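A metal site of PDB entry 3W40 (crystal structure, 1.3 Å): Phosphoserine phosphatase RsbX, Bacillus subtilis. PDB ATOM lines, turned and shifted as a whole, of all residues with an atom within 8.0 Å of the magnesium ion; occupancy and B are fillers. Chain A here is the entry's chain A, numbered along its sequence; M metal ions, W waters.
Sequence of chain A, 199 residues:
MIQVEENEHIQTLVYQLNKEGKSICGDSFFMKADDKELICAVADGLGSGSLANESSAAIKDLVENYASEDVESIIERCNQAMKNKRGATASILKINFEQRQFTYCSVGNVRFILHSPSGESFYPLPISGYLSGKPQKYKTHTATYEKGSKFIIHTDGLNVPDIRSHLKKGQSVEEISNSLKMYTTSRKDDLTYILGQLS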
ATOM      1  N   LYS A  22      12.284 -18.247   1.162  1.00  0.00           N
ATOM      2  CA  LYS A  22      11.568 -19.186   2.067  1.00  0.00           C
ATOM      3  C   LYS A  22      11.855 -20.604   1.555  1.00  0.00           C
ATOM      4  O   LYS A  22      11.602 -20.911   0.384  1.00  0.00           O
ATOM      5  CB  LYS A  22      10.051 -18.833   2.116  1.00  0.00           C
ATOM      6  CG  LYS A  22       9.052 -19.679   2.976  1.00  0.00           C
ATOM      7  CD  LYS A  22       7.545 -19.568   2.458  1.00  0.00           C
ATOM      8  CE  LYS A  22       6.596 -20.149   3.473  1.00  0.00           C
ATOM      9  NZ  LYS A  22       5.203 -19.572   3.390  1.00  0.00           N
ATOM     10  N   GLY A  26       4.329 -23.348   1.943  1.00  0.00           N
ATOM     11  CA  GLY A  26       3.129 -23.574   2.727  1.00  0.00           C
ATOM     12  C   GLY A  26       1.929 -24.026   1.864  1.00  0.00           C
ATOM     13  O   GLY A  26       0.925 -24.421   2.418  1.00  0.00           O
ATOM     14  N   ASP A  27       2.050 -23.971   0.516  1.00  0.00           N
ATOM     15  CA  ASP A  27       0.972 -24.352  -0.396  1.00  0.00           C
ATOM     16  C   ASP A  27       1.246 -25.813  -0.806  1.00  0.00           C
ATOM     17  O   ASP A  27       2.383 -26.251  -0.834  1.00  0.00           O
ATOM     18  CB  ASP A  27       1.147 -23.561  -1.706  1.00  0.00           C
ATOM     19  CG  ASP A  27       0.652 -22.089  -1.669  1.00  0.00           C
ATOM     20  OD1 ASP A  27       0.227 -21.589  -0.640  1.00  0.00           O
ATOM     21  OD2 ASP A  27       0.778 -21.456  -2.770  1.00  0.00           O
ATOM     22  N   ALA A  43      -4.192 -26.123  -1.880  1.00  0.00           N
ATOM     23  CA  ALA A  43      -4.391 -25.748  -0.489  1.00  0.00           C
ATOM     24  C   ALA A  43      -3.294 -24.838  -0.026  1.00  0.00           C
ATOM     25  O   ALA A  43      -2.176 -24.943  -0.534  1.00  0.00           O
ATOM     26  CB  ALA A  43      -4.456 -26.975   0.431  1.00  0.00           C
ATOM     27  N   ASP A  44      -3.580 -23.966   0.918  1.00  0.00           N
ATOM     28  CA  ASP A  44      -2.626 -22.989   1.452  1.00  0.00           C
ATOM     29  C   ASP A  44      -2.706 -23.092   2.987  1.00  0.00           C
ATOM     30  O   ASP A  44      -3.763 -22.783   3.580  1.00  0.00           O
ATOM     31  CB  ASP A  44      -2.986 -21.575   0.923  1.00  0.00           C
ATOM     32  CG  ASP A  44      -2.013 -20.477   1.410  1.00  0.00           C
ATOM     33  OD1 ASP A  44      -1.158 -20.762   2.292  1.00  0.00           O
ATOM     34  OD2 ASP A  44      -2.126 -19.298   0.953  1.00  0.00           O
ATOM     35  N   GLY A  45      -1.657 -23.628   3.602  1.00  0.00           N
ATOM     36  CA  GLY A  45      -1.690 -23.842   5.050  1.00  0.00           C
ATOM     37  C   GLY A  45      -1.624 -22.532   5.838  1.00  0.00           C
ATOM     38  O   GLY A  45      -0.971 -21.561   5.419  1.00  0.00           O
ATOM     39  N   THR A  89      -6.607 -23.155   3.878  1.00  0.00           N
ATOM     40  CA  THR A  89      -7.643 -22.864   2.889  1.00  0.00           C
ATOM     41  C   THR A  89      -7.462 -23.863   1.739  1.00  0.00           C
ATOM     42  O   THR A  89      -6.344 -24.328   1.504  1.00  0.00           O
ATOM     43  CB  THR A  89      -7.555 -21.421   2.437  1.00  0.00           C
ATOM     44  OG1 THR A  89      -6.283 -21.170   1.841  1.00  0.00           O
ATOM     45  CG2 THR A  89      -7.789 -20.491   3.584  1.00  0.00           C
ATOM     46  N   ASN A 109      -9.641 -18.913   0.705  1.00  0.00           N
ATOM     47  CA  ASN A 109      -9.259 -17.914  -0.262  1.00  0.00           C
ATOM     48  C   ASN A 109      -8.498 -18.494  -1.445  1.00  0.00           C
ATOM     49  O   ASN A 109      -7.912 -17.708  -2.183  1.00  0.00           O
ATOM     50  CB  ASN A 109      -8.520 -16.775   0.369  1.00  0.00           C
ATOM     51  CG  ASN A 109      -7.125 -17.122   0.860  1.00  0.00           C
ATOM     52  OD1 ASN A 109      -6.409 -16.198   1.202  1.00  0.00           O
ATOM     53  ND2 ASN A 109      -6.749 -18.401   0.907  1.00  0.00           N
ATOM     54  N   VAL A 110      -8.574 -19.806  -1.677  1.00  0.00           N
ATOM     55  CA  VAL A 110      -8.042 -20.392  -2.885  1.00  0.00           C
ATOM     56  C   VAL A 110      -9.118 -20.234  -3.930  1.00  0.00           C
ATOM     57  O   VAL A 110     -10.253 -20.604  -3.697  1.00  0.00           O
ATOM     58  CB  VAL A 110      -7.678 -21.903  -2.652  1.00  0.00           C
ATOM     59  CG1 VAL A 110      -7.202 -22.496  -3.924  1.00  0.00           C
ATOM     60  CG2 VAL A 110      -6.593 -22.009  -1.612  1.00  0.00           C
ATOM     61  N   THR A 155      -3.760 -20.072  -5.375  1.00  0.00           N
ATOM     62  CA  THR A 155      -3.649 -19.556  -4.053  1.00  0.00           C
ATOM     63  C   THR A 155      -3.572 -18.022  -4.100  1.00  0.00           C
ATOM     64  O   THR A 155      -3.379 -17.370  -5.148  1.00  0.00           O
ATOM     65  CB  THR A 155      -2.462 -20.157  -3.278  1.00  0.00           C
ATOM     66  OG1 THR A 155      -1.269 -19.822  -3.954  1.00  0.00           O
ATOM     67  CG2 THR A 155      -2.678 -21.604  -3.138  1.00  0.00           C
ATOM     68  N   ASP A 156      -3.636 -17.466  -2.912  1.00  0.00           N
ATOM     69  CA  ASP A 156      -3.593 -15.991  -2.753  1.00  0.00           C
ATOM     70  C   ASP A 156      -2.268 -15.338  -3.097  1.00  0.00           C
ATOM     71  O   ASP A 156      -2.194 -14.138  -3.200  1.00  0.00           O
ATOM     72  CB  ASP A 156      -4.076 -15.551  -1.384  1.00  0.00           C
ATOM     73  CG  ASP A 156      -3.211 -16.075  -0.249  1.00  0.00           C
ATOM     74  OD1 ASP A 156      -2.191 -16.767  -0.469  1.00  0.00           O
ATOM     75  OD2 ASP A 156      -3.497 -15.680   0.933  1.00  0.00           O
ATOM     76  N   GLY A 157      -1.232 -16.145  -3.319  1.00  0.00           N
ATOM     77  CA  GLY A 157       0.031 -15.608  -3.832  1.00  0.00           C
ATOM     78  C   GLY A 157      -0.083 -15.062  -5.251  1.00  0.00           C
ATOM     79  O   GLY A 157       0.767 -14.256  -5.646  1.00  0.00           O
ATOM     80  N   LEU A 158      -1.138 -15.470  -5.991  1.00  0.00           N
ATOM     81  CA  LEU A 158      -1.346 -14.940  -7.344  1.00  0.00           C
ATOM     82  C   LEU A 158      -2.408 -13.869  -7.278  1.00  0.00           C
ATOM     83  O   LEU A 158      -3.535 -14.170  -6.908  1.00  0.00           O
ATOM     84  CB  LEU A 158      -1.768 -16.067  -8.264  1.00  0.00           C
ATOM     85  CG  LEU A 158      -2.013 -15.614  -9.719  1.00  0.00           C
ATOM     86  CD1 LEU A 158      -0.781 -15.145 -10.443  1.00  0.00           C
ATOM     87  CD2 LEU A 158      -2.651 -16.723 -10.517  1.00  0.00           C
ATOM     88  N   LYS A 188       6.139 -12.342  -3.265  1.00  0.00           N
ATOM     89  CA  LYS A 188       5.713 -11.870  -1.930  1.00  0.00           C
ATOM     90  C   LYS A 188       5.111 -12.976  -1.051  1.00  0.00           C
ATOM     91  O   LYS A 188       5.158 -12.891   0.173  1.00  0.00           O
ATOM     92  CB  LYS A 188       4.669 -10.777  -2.088  1.00  0.00           C
ATOM     93  CG  LYS A 188       4.518  -9.862  -0.890  1.00  0.00           C
ATOM     94  CD  LYS A 188       4.020  -8.510  -1.375  1.00  0.00           C
ATOM     95  CE  LYS A 188       5.003  -7.867  -2.380  1.00  0.00           C
ATOM     96  NZ  LYS A 188       5.923  -6.877  -1.761  1.00  0.00           N
ATOM     97  N   ASP A 189       4.504 -13.995  -1.668  1.00  0.00           N
ATOM     98  CA  ASP A 189       3.952 -15.126  -0.944  1.00  0.00           C
ATOM     99  C   ASP A 189       4.250 -16.342  -1.797  1.00  0.00           C
ATOM    100  O   ASP A 189       4.575 -16.194  -2.966  1.00  0.00           O
ATOM    101  CB  ASP A 189       2.443 -14.972  -0.815  1.00  0.00           C
ATOM    102  CG  ASP A 189       1.794 -16.038   0.130  1.00  0.00           C
ATOM    103  OD1 ASP A 189       2.546 -16.748   0.864  1.00  0.00           O
ATOM    104  OD2 ASP A 189       0.542 -16.179   0.082  1.00  0.00           O
ATOM    105  N   ASP A 190       4.115 -17.534  -1.215  1.00  0.00           N
ATOM    106  CA  ASP A 190       4.041 -18.765  -2.053  1.00  0.00           C
ATOM    107  C   ASP A 190       2.950 -18.597  -3.103  1.00  0.00           C
ATOM    108  O   ASP A 190       1.911 -18.025  -2.798  1.00  0.00           O
ATOM    109  CB  ASP A 190       3.658 -19.943  -1.189  1.00  0.00           C
ATOM    110  CG  ASP A 190       4.695 -20.229  -0.088  1.00  0.00           C
ATOM    111  OD1 ASP A 190       5.908 -20.002  -0.270  1.00  0.00           O
ATOM    112  OD2 ASP A 190       4.288 -20.710   0.998  1.00  0.00           O
ATOM    113  N   LEU A 191       3.192 -19.101  -4.321  1.00  0.00           N
ATOM    114  CA  LEU A 191       2.248 -18.876  -5.412  1.00  0.00           C
ATOM    115  C   LEU A 191       2.080 -20.224  -6.078  1.00  0.00           C
ATOM    116  O   LEU A 191       3.069 -20.794  -6.557  1.00  0.00           O
ATOM    117  CB  LEU A 191       2.850 -17.819  -6.342  1.00  0.00           C
ATOM    118  CG  LEU A 191       1.970 -17.231  -7.461  1.00  0.00           C
ATOM    119  CD1 LEU A 191       2.547 -15.970  -8.022  1.00  0.00           C
ATOM    120  CD2 LEU A 191       1.672 -18.184  -8.602  1.00  0.00           C
ATOM    121  N   THR A 192       0.837 -20.705  -6.126  1.00  0.00           N
ATOM    122  CA  THR A 192       0.506 -21.994  -6.751  1.00  0.00           C
ATOM    123  C   THR A 192      -0.703 -21.821  -7.633  1.00  0.00           C
ATOM    124  O   THR A 192      -1.661 -21.181  -7.226  1.00  0.00           O
ATOM    125  CB  THR A 192       0.180 -23.061  -5.713  1.00  0.00           C
ATOM    126  OG1 THR A 192       1.281 -23.200  -4.816  1.00  0.00           O
ATOM    127  CG2 THR A 192      -0.060 -24.424  -6.343  1.00  0.00           C
HETATM  128 MG    MG M   1      -0.772 -17.705   0.591  1.00  0.00          MG
HETATM  129  O   HOH W   1      -1.452 -16.652   2.325  1.00  0.00           O
HETATM  130  O   HOH W   2      -0.062 -18.843  -0.991  1.00  0.00           O
HETATM  131  O   HOH W   3       0.707 -18.398   1.884  1.00  0.00           O
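OD1 of Asp 156 binds the magnesium ion (2.0 Å). The magnesium ion is bound by water W2 (2.1 Å). The magnesium ion is bound by OD2 of Asp 189, 2.1 Å away. Water W3 binds the magnesium ion (2.1 Å). OD2 of Asp 44 binds the magnesium ion (2.1 Å). The magnesium ion is bound by water W1, 2.1 Å away.
Water W3 bridges the side-chain carboxylate of Asp 189 (2.7 Å) and the side-chain carboxylate of Asp 44 (3.0 Å). Water W2 lies within hydrogen-bond range of the side-chain carboxylate of Asp 27 (2.8 Å), the backbone carbonyl oxygen of Asp 190 (2.8 Å) and the side-chain hydroxyl of Thr 155 (3.3 Å).
The nearest printed residue that does not touch the magnesium ion is Asp 27 (4.2 Å).
OD1 of Asn 109 sits close to OD2 of Asp 156 (3.0 Å). The backbone NH (N) of Asp 44 lies within hydrogen-bond range of the backbone carbonyl oxygen (O) of Thr 89 (2.8 Å).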
